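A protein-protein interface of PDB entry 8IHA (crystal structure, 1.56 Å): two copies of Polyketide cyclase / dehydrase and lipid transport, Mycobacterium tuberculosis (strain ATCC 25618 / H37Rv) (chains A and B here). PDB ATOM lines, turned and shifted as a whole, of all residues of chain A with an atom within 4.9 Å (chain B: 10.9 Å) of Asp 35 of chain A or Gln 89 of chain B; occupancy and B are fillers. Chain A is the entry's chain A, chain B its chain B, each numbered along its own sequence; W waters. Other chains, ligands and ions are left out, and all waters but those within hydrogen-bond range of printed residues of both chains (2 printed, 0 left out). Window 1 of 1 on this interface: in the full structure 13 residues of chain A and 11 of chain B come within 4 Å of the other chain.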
ATOM      1  N   TRP A  33       7.618 -18.984 -31.785  1.00  0.00           N
ATOM      2  CA  TRP A  33       7.575 -20.323 -31.171  1.00  0.00           C
ATOM      3  C   TRP A  33       8.199 -20.263 -29.803  1.00  0.00           C
ATOM      4  O   TRP A  33       9.249 -20.824 -29.575  1.00  0.00           O
ATOM      5  CB  TRP A  33       8.323 -21.299 -32.091  1.00  0.00           C
ATOM      6  CG  TRP A  33       7.712 -21.377 -33.457  1.00  0.00           C
ATOM      7  CD1 TRP A  33       6.449 -21.837 -33.762  1.00  0.00           C
ATOM      8  CD2 TRP A  33       8.311 -20.988 -34.693  1.00  0.00           C
ATOM      9  NE1 TRP A  33       6.226 -21.711 -35.105  1.00  0.00           N
ATOM     10  CE2 TRP A  33       7.355 -21.205 -35.721  1.00  0.00           C
ATOM     11  CE3 TRP A  33       9.566 -20.504 -35.043  1.00  0.00           C
ATOM     12  CZ2 TRP A  33       7.617 -20.955 -37.053  1.00  0.00           C
ATOM     13  CZ3 TRP A  33       9.845 -20.296 -36.357  1.00  0.00           C
ATOM     14  CH2 TRP A  33       8.881 -20.513 -37.367  1.00  0.00           C
ATOM     15  N   PRO A  34       7.610 -19.520 -28.846  1.00  0.00           N
ATOM     16  CA  PRO A  34       8.251 -19.382 -27.548  1.00  0.00           C
ATOM     17  C   PRO A  34       8.454 -20.658 -26.742  1.00  0.00           C
ATOM     18  O   PRO A  34       9.378 -20.676 -25.896  1.00  0.00           O
ATOM     19  CB  PRO A  34       7.288 -18.423 -26.840  1.00  0.00           C
ATOM     20  CG  PRO A  34       6.034 -18.433 -27.564  1.00  0.00           C
ATOM     21  CD  PRO A  34       6.388 -18.737 -28.995  1.00  0.00           C
ATOM     22  N   ASP A  35       7.662 -21.688 -27.006  1.00  0.00           N
ATOM     23  CA  ASP A  35       7.846 -22.982 -26.272  1.00  0.00           C
ATOM     24  C   ASP A  35       8.710 -23.968 -27.054  1.00  0.00           C
ATOM     25  O   ASP A  35       8.859 -25.086 -26.570  1.00  0.00           O
ATOM     26  CB  ASP A  35       6.506 -23.564 -25.859  1.00  0.00           C
ATOM     27  CG  ASP A  35       5.718 -24.255 -26.939  1.00  0.00           C
ATOM     28  OD1 ASP A  35       6.050 -24.064 -28.119  1.00  0.00           O
ATOM     29  OD2 ASP A  35       4.677 -24.851 -26.590  1.00  0.00           O
ATOM     30  N   LEU A  36       9.305 -23.557 -28.164  1.00  0.00           N
ATOM     31  CA  LEU A  36      10.216 -24.426 -28.944  1.00  0.00           C
ATOM     32  C   LEU A  36      11.624 -23.889 -28.877  1.00  0.00           C
ATOM     33  O   LEU A  36      11.809 -22.657 -28.777  1.00  0.00           O
ATOM     34  CB  LEU A  36       9.780 -24.545 -30.398  1.00  0.00           C
ATOM     35  CG  LEU A  36       8.376 -25.059 -30.685  1.00  0.00           C
ATOM     36  CD1 LEU A  36       8.112 -25.225 -32.179  1.00  0.00           C
ATOM     37  CD2 LEU A  36       8.062 -26.340 -29.916  1.00  0.00           C
ATOM     38  N   ARG A  37      12.626 -24.762 -29.010  1.00  0.00           N
ATOM     39  CA  ARG A  37      14.040 -24.423 -29.208  1.00  0.00           C
ATOM     40  C   ARG A  37      14.437 -25.000 -30.547  1.00  0.00           C
ATOM     41  O   ARG A  37      14.214 -26.192 -30.783  1.00  0.00           O
ATOM     42  CB  ARG A  37      14.947 -24.908 -28.058  1.00  0.00           C
ATOM     43  CG  ARG A  37      14.646 -24.224 -26.733  1.00  0.00           C
ATOM     44  CD  ARG A  37      15.576 -24.645 -25.602  1.00  0.00           C
ATOM     45  NE  ARG A  37      15.386 -26.040 -25.333  1.00  0.00           N
ATOM     46  CZ  ARG A  37      14.403 -26.564 -24.639  1.00  0.00           C
ATOM     47  NH1 ARG A  37      13.450 -25.815 -24.093  1.00  0.00           N
ATOM     48  NH2 ARG A  37      14.367 -27.886 -24.501  1.00  0.00           N
ATOM     49  N   THR A  54      13.231 -28.933 -30.489  1.00  0.00           N
ATOM     50  CA  THR A  54      13.190 -29.450 -29.102  1.00  0.00           C
ATOM     51  C   THR A  54      12.331 -28.500 -28.293  1.00  0.00           C
ATOM     52  O   THR A  54      11.767 -27.565 -28.894  1.00  0.00           O
ATOM     53  CB  THR A  54      14.579 -29.629 -28.514  1.00  0.00           C
ATOM     54  OG1 THR A  54      15.285 -28.384 -28.475  1.00  0.00           O
ATOM     55  CG2 THR A  54      15.365 -30.650 -29.302  1.00  0.00           C
ATOM     56  N   GLY A  55      12.241 -28.703 -26.985  1.00  0.00           N
ATOM     57  CA  GLY A  55      11.328 -27.924 -26.147  1.00  0.00           C
ATOM     58  C   GLY A  55      10.028 -28.662 -26.035  1.00  0.00           C
ATOM     59  O   GLY A  55      10.044 -29.898 -25.782  1.00  0.00           O
ATOM     60  N   ALA A  56       8.883 -28.036 -26.271  1.00  0.00           N
ATOM     61  CA  ALA A  56       7.559 -28.638 -26.056  1.00  0.00           C
ATOM     62  C   ALA A  56       7.289 -29.746 -27.074  1.00  0.00           C
ATOM     63  O   ALA A  56       6.483 -30.599 -26.783  1.00  0.00           O
ATOM     64  CB  ALA A  56       6.451 -27.619 -26.108  1.00  0.00           C
ATOM     65  N   ARG A 102      -0.816 -25.259 -33.433  1.00  0.00           N
ATOM     66  CA  ARG A 102       0.514 -25.110 -34.099  1.00  0.00           C
ATOM     67  C   ARG A 102       0.344 -24.551 -35.519  1.00  0.00           C
ATOM     68  O   ARG A 102       1.223 -23.807 -36.011  1.00  0.00           O
ATOM     69  CB  ARG A 102       1.224 -26.455 -34.143  1.00  0.00           C
ATOM     70  CG  ARG A 102       1.547 -27.019 -32.780  1.00  0.00           C
ATOM     71  CD  ARG A 102       2.481 -26.255 -31.959  1.00  0.00           C
ATOM     72  NE  ARG A 102       2.751 -26.763 -30.647  1.00  0.00           N
ATOM     73  CZ  ARG A 102       3.631 -26.217 -29.807  1.00  0.00           C
ATOM     74  NH1 ARG A 102       4.370 -25.174 -30.165  1.00  0.00           N
ATOM     75  NH2 ARG A 102       3.791 -26.767 -28.628  1.00  0.00           N
ATOM     76  N   SER B   3      12.705 -23.026  -8.863  1.00  0.00           N
ATOM     77  CA  SER B   3      11.889 -21.929  -9.434  1.00  0.00           C
ATOM     78  C   SER B   3      10.437 -22.100  -8.960  1.00  0.00           C
ATOM     79  O   SER B   3       9.744 -21.076  -8.814  1.00  0.00           O
ATOM     80  CB  SER B   3      11.960 -21.837 -10.951  1.00  0.00           C
ATOM     81  OG  SER B   3      13.281 -21.638 -11.425  1.00  0.00           O
ATOM     82  N   ALA B  56       6.922 -31.744 -17.432  1.00  0.00           N
ATOM     83  CA  ALA B  56       6.841 -30.260 -17.520  1.00  0.00           C
ATOM     84  C   ALA B  56       7.810 -29.624 -16.523  1.00  0.00           C
ATOM     85  O   ALA B  56       8.369 -28.567 -16.833  1.00  0.00           O
ATOM     86  CB  ALA B  56       5.448 -29.842 -17.283  1.00  0.00           C
ATOM     87  N   GLU B  81      12.014 -27.166 -11.408  1.00  0.00           N
ATOM     88  CA  GLU B  81      12.338 -26.113 -12.393  1.00  0.00           C
ATOM     89  C   GLU B  81      11.713 -26.522 -13.713  1.00  0.00           C
ATOM     90  O   GLU B  81      11.654 -27.712 -14.050  1.00  0.00           O
ATOM     91  CB  GLU B  81      13.851 -25.977 -12.519  1.00  0.00           C
ATOM     92  CG  GLU B  81      14.509 -25.243 -11.361  1.00  0.00           C
ATOM     93  CD  GLU B  81      16.039 -25.265 -11.293  1.00  0.00           C
ATOM     94  OE1 GLU B  81      16.718 -25.764 -12.240  1.00  0.00           O
ATOM     95  OE2 GLU B  81      16.577 -24.754 -10.251  1.00  0.00           O
ATOM     96  N   PRO B  82      11.231 -25.550 -14.505  1.00  0.00           N
ATOM     97  CA  PRO B  82      10.712 -25.840 -15.837  1.00  0.00           C
ATOM     98  C   PRO B  82      11.753 -26.588 -16.658  1.00  0.00           C
ATOM     99  O   PRO B  82      12.876 -26.171 -16.816  1.00  0.00           O
ATOM    100  CB  PRO B  82      10.413 -24.454 -16.415  1.00  0.00           C
ATOM    101  CG  PRO B  82      10.233 -23.577 -15.213  1.00  0.00           C
ATOM    102  CD  PRO B  82      11.191 -24.114 -14.181  1.00  0.00           C
ATOM    103  N   THR B  83      11.352 -27.731 -17.204  1.00  0.00           N
ATOM    104  CA  THR B  83      12.307 -28.717 -17.722  1.00  0.00           C
ATOM    105  C   THR B  83      13.070 -28.263 -18.975  1.00  0.00           C
ATOM    106  O   THR B  83      12.385 -27.913 -19.919  1.00  0.00           O
ATOM    107  CB  THR B  83      11.550 -29.982 -18.101  1.00  0.00           C
ATOM    108  OG1 THR B  83      11.138 -30.537 -16.842  1.00  0.00           O
ATOM    109  CG2 THR B  83      12.382 -30.961 -18.909  1.00  0.00           C
ATOM    110  N   GLY B  84      14.404 -28.204 -18.928  1.00  0.00           N
ATOM    111  CA  GLY B  84      15.281 -28.008 -20.109  1.00  0.00           C
ATOM    112  C   GLY B  84      15.135 -26.613 -20.719  1.00  0.00           C
ATOM    113  O   GLY B  84      15.636 -26.441 -21.857  1.00  0.00           O
ATOM    114  N   VAL B  85      14.533 -25.645 -20.015  1.00  0.00           N
ATOM    115  CA  VAL B  85      14.220 -24.343 -20.677  1.00  0.00           C
ATOM    116  C   VAL B  85      15.514 -23.555 -20.836  1.00  0.00           C
ATOM    117  O   VAL B  85      16.468 -23.677 -20.052  1.00  0.00           O
ATOM    118  CB  VAL B  85      13.132 -23.475 -20.025  1.00  0.00           C
ATOM    119  CG1 VAL B  85      11.746 -24.098 -20.153  1.00  0.00           C
ATOM    120  CG2 VAL B  85      13.473 -23.118 -18.613  1.00  0.00           C
ATOM    121  N   ALA B  86      15.548 -22.756 -21.892  1.00  0.00           N
ATOM    122  CA  ALA B  86      16.623 -21.772 -22.103  1.00  0.00           C
ATOM    123  C   ALA B  86      16.309 -20.530 -21.276  1.00  0.00           C
ATOM    124  O   ALA B  86      15.181 -20.336 -20.833  1.00  0.00           O
ATOM    125  CB  ALA B  86      16.769 -21.471 -23.564  1.00  0.00           C
ATOM    126  N   ALA B  87      17.362 -19.766 -21.008  1.00  0.00           N
ATOM    127  CA  ALA B  87      17.252 -18.541 -20.194  1.00  0.00           C
ATOM    128  C   ALA B  87      16.199 -17.625 -20.824  1.00  0.00           C
ATOM    129  O   ALA B  87      15.398 -17.060 -20.052  1.00  0.00           O
ATOM    130  CB  ALA B  87      18.580 -17.830 -20.060  1.00  0.00           C
ATOM    131  N   TRP B  88      16.123 -17.570 -22.168  1.00  0.00           N
ATOM    132  CA  TRP B  88      15.163 -16.659 -22.850  1.00  0.00           C
ATOM    133  C   TRP B  88      13.740 -17.132 -22.590  1.00  0.00           C
ATOM    134  O   TRP B  88      12.815 -16.289 -22.468  1.00  0.00           O
ATOM    135  CB  TRP B  88      15.515 -16.463 -24.322  1.00  0.00           C
ATOM    136  CG  TRP B  88      15.346 -17.642 -25.219  1.00  0.00           C
ATOM    137  CD1 TRP B  88      16.288 -18.544 -25.637  1.00  0.00           C
ATOM    138  CD2 TRP B  88      14.113 -18.053 -25.815  1.00  0.00           C
ATOM    139  NE1 TRP B  88      15.704 -19.476 -26.453  1.00  0.00           N
ATOM    140  CE2 TRP B  88      14.378 -19.212 -26.549  1.00  0.00           C
ATOM    141  CE3 TRP B  88      12.807 -17.573 -25.775  1.00  0.00           C
ATOM    142  CZ2 TRP B  88      13.397 -19.842 -27.326  1.00  0.00           C
ATOM    143  CZ3 TRP B  88      11.834 -18.222 -26.508  1.00  0.00           C
ATOM    144  CH2 TRP B  88      12.127 -19.346 -27.258  1.00  0.00           C
ATOM    145  N   GLN B  89      13.492 -18.451 -22.436  1.00  0.00           N
ATOM    146  CA  GLN B  89      12.132 -18.945 -22.158  1.00  0.00           C
ATOM    147  C   GLN B  89      11.789 -18.651 -20.696  1.00  0.00           C
ATOM    148  O   GLN B  89      10.639 -18.271 -20.369  1.00  0.00           O
ATOM    149  CB  GLN B  89      12.129 -20.459 -22.437  1.00  0.00           C
ATOM    150  CG  GLN B  89      12.397 -20.751 -23.922  1.00  0.00           C
ATOM    151  CD  GLN B  89      12.376 -22.225 -24.205  1.00  0.00           C
ATOM    152  OE1 GLN B  89      13.265 -22.959 -23.774  1.00  0.00           O
ATOM    153  NE2 GLN B  89      11.420 -22.637 -25.008  1.00  0.00           N
ATOM    154  N   LEU B  90      12.743 -18.883 -19.786  1.00  0.00           N
ATOM    155  CA  LEU B  90      12.472 -18.671 -18.333  1.00  0.00           C
ATOM    156  C   LEU B  90      12.092 -17.205 -18.112  1.00  0.00           C
ATOM    157  O   LEU B  90      11.117 -16.961 -17.416  1.00  0.00           O
ATOM    158  CB  LEU B  90      13.723 -19.051 -17.541  1.00  0.00           C
ATOM    159  CG  LEU B  90      13.610 -18.917 -16.022  1.00  0.00           C
ATOM    160  CD1 LEU B  90      12.705 -19.989 -15.431  1.00  0.00           C
ATOM    161  CD2 LEU B  90      14.996 -18.984 -15.404  1.00  0.00           C
ATOM    162  N   ALA B  91      12.727 -16.306 -18.838  1.00  0.00           N
ATOM    163  CA  ALA B  91      12.470 -14.834 -18.735  1.00  0.00           C
ATOM    164  C   ALA B  91      11.037 -14.463 -19.101  1.00  0.00           C
ATOM    165  O   ALA B  91      10.587 -13.425 -18.619  1.00  0.00           O
ATOM    166  CB  ALA B  91      13.396 -14.053 -19.631  1.00  0.00           C
ATOM    167  N   ARG B  92      10.376 -15.245 -19.949  1.00  0.00           N
ATOM    168  CA  ARG B  92       8.997 -15.002 -20.423  1.00  0.00           C
ATOM    169  C   ARG B  92       7.993 -15.651 -19.467  1.00  0.00           C
ATOM    170  O   ARG B  92       6.785 -15.450 -19.691  1.00  0.00           O
ATOM    171  CB  ARG B  92       8.802 -15.589 -21.827  1.00  0.00           C
ATOM    172  CG  ARG B  92       9.583 -14.925 -22.947  1.00  0.00           C
ATOM    173  CD  ARG B  92       9.625 -15.851 -24.171  1.00  0.00           C
ATOM    174  NE  ARG B  92       9.976 -15.165 -25.407  1.00  0.00           N
ATOM    175  CZ  ARG B  92       9.094 -14.595 -26.225  1.00  0.00           C
ATOM    176  NH1 ARG B  92       7.798 -14.619 -25.936  1.00  0.00           N
ATOM    177  NH2 ARG B  92       9.525 -13.955 -27.295  1.00  0.00           N
ATOM    178  N   MET B  93       8.430 -16.449 -18.488  1.00  0.00           N
ATOM    179  CA  MET B  93       7.445 -17.156 -17.623  1.00  0.00           C
ATOM    180  C   MET B  93       7.067 -16.273 -16.434  1.00  0.00           C
ATOM    181  O   MET B  93       7.920 -15.581 -15.922  1.00  0.00           O
ATOM    182  CB  MET B  93       7.977 -18.500 -17.125  1.00  0.00           C
ATOM    183  CG  MET B  93       8.091 -19.463 -18.215  1.00  0.00           C
ATOM    184  SD  MET B  93       9.011 -20.921 -17.709  1.00  0.00           S
ATOM    185  CE  MET B  93       9.161 -21.708 -19.302  1.00  0.00           C
ATOM    186  N   ASN B  94       5.798 -16.372 -16.026  1.00  0.00           N
ATOM    187  CA  ASN B  94       5.284 -15.762 -14.781  1.00  0.00           C
ATOM    188  C   ASN B  94       5.389 -16.860 -13.711  1.00  0.00           C
ATOM    189  O   ASN B  94       4.427 -17.640 -13.560  1.00  0.00           O
ATOM    190  CB  ASN B  94       3.847 -15.248 -14.949  1.00  0.00           C
ATOM    191  CG  ASN B  94       3.297 -14.593 -13.700  1.00  0.00           C
ATOM    192  OD1 ASN B  94       3.789 -14.818 -12.592  1.00  0.00           O
ATOM    193  ND2 ASN B  94       2.303 -13.737 -13.873  1.00  0.00           N
ATOM    194  N   LEU B  95       6.540 -16.954 -13.049  1.00  0.00           N
ATOM    195  CA  LEU B  95       6.722 -18.041 -12.050  1.00  0.00           C
ATOM    196  C   LEU B  95       5.716 -17.924 -10.900  1.00  0.00           C
ATOM    197  O   LEU B  95       5.395 -18.978 -10.322  1.00  0.00           O
ATOM    198  CB  LEU B  95       8.160 -18.055 -11.545  1.00  0.00           C
ATOM    199  CG  LEU B  95       9.215 -18.351 -12.614  1.00  0.00           C
ATOM    200  CD1 LEU B  95      10.596 -18.296 -11.980  1.00  0.00           C
ATOM    201  CD2 LEU B  95       8.987 -19.688 -13.330  1.00  0.00           C
ATOM    202  N   ARG B  97       2.499 -17.022 -11.093  1.00  0.00           N
ATOM    203  CA  ARG B  97       1.237 -17.568 -11.643  1.00  0.00           C
ATOM    204  C   ARG B  97       1.409 -19.095 -11.666  1.00  0.00           C
ATOM    205  O   ARG B  97       0.492 -19.794 -11.302  1.00  0.00           O
ATOM    206  CB  ARG B  97       0.961 -16.969 -13.033  1.00  0.00           C
ATOM    207  CG  ARG B  97      -0.399 -17.314 -13.629  1.00  0.00           C
ATOM    208  CD  ARG B  97      -0.467 -17.127 -15.145  1.00  0.00           C
ATOM    209  NE  ARG B  97       0.592 -17.967 -15.718  1.00  0.00           N
ATOM    210  CZ  ARG B  97       0.443 -19.169 -16.276  1.00  0.00           C
ATOM    211  NH1 ARG B  97      -0.752 -19.701 -16.467  1.00  0.00           N
ATOM    212  NH2 ARG B  97       1.513 -19.814 -16.709  1.00  0.00           N
ATOM    213  N   MET B  98       2.566 -19.551 -12.128  1.00  0.00           N
ATOM    214  CA  MET B  98       2.833 -20.995 -12.305  1.00  0.00           C
ATOM    215  C   MET B  98       2.780 -21.655 -10.930  1.00  0.00           C
ATOM    216  O   MET B  98       2.098 -22.734 -10.779  1.00  0.00           O
ATOM    217  CB  MET B  98       4.205 -21.190 -12.938  1.00  0.00           C
ATOM    218  CG  MET B  98       4.164 -20.873 -14.428  1.00  0.00           C
ATOM    219  SD  MET B  98       5.823 -20.806 -15.194  1.00  0.00           S
ATOM    220  CE  MET B  98       6.233 -22.554 -15.202  1.00  0.00           C
HETATM  221  O   HOH W   1      12.292 -28.084 -22.654  1.00  0.00           O
HETATM  222  O   HOH W   2       9.846 -25.405 -23.921  1.00  0.00           O
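The backbone carbonyl oxygen of Pro 34 of chain A is in hydrogen-bond range of the side-chain amide nitrogen of Gln 89 of chain B, 3.0 Å away.
NH1 of Arg 37 of chain A is in hydrogen-bond range of OE1 of Gln 89 of chain B, 2.9 Å away.
NH1 of Arg 37 of chain A sits close to O of Gly 84 of chain B, at 3.2 Å.
The side-chain carboxylate (OD1) of Asp 35 of chain A is in salt-bridge range of the guanidinium group (NH1) of Arg 102 of chain A.
The side-chain amide oxygen (OE1) of Gln 89 of chain B lies within hydrogen-bond range of the backbone NH (N) of Ala 86 of chain B, 3.0 Å away.
The backbone carbonyl oxygen of Arg 37 of chain A sits at hydrogen-bond distance from the backbone NH of Thr 54 of chain A (2.9 Å).
O of Asp 35 of chain A lies within hydrogen-bond range of N of Ala 56 of chain A, at 3.0 Å.
Among the printed residues, pairs that only touch across the chains: Pro 34 of chain A with Trp 88 of chain B, Leu 36 of chain A with Trp 88 of chain B, Asp 35 of chain A with Gln 89 of chain B, Leu 36 of chain A with Gln 89 of chain B, Arg 37 of chain A with Val 85 of chain B, Pro 34 of chain A with Arg 92 of chain B, Arg 37 of chain A with Ala 86 of chain B and Trp 33 of chain A with Trp 88 of chain B.
Asp 35 of chain A touches one residue of chain B.
No residue of chain B comes within 4 Å of Gly 55 of chain A.
Printed residues of chain A within 4 Å of Ala 86 of chain B: Arg 37 (3.96 Å).
Of the printed residues of chain A, Val 85 of chain B touches Arg 37 (3.8 Å).
Met 93 of chain B touches none of the printed residues of chain A.
Ala 91 of chain B touches none of the printed residues of chain A.
The nearest printed residue of chain A that does not touch Gln 89 of chain B is Trp 33 of chain A (5.4 Å).
Of the 9 printed residues of chain A, 5 touch a printed residue of chain B.
Of the 19 printed residues of chain B, 6 touch a printed residue of chain A.
Hydrophobic or aromatic side chains of chain B that line the printed part of chain A: Ala 86 and Trp 88.
Among the printed residues, 11 pairs touch across the chains.
Among the printed residues, no Asp or Glu carboxylate lies within 4 Å of a Lys or Arg side-chain nitrogen of the other chain.
1 position is printed for both chains.
Of the 11 pairs that touch across the chains among the printed residues, none has its exchanged pair printed and touching as well.
Water W1 lies within hydrogen-bond range of the backbone carbonyl oxygen of Thr 83 of chain B (2.7 Å) and the guanidinium group of Arg 37 of chain A (2.8 Å).
Water W2 bridges the backbone carbonyl oxygen of Asp 35 of chain A (2.8 Å) and the side-chain amide nitrogen of Gln 89 of chain B (3.4 Å).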
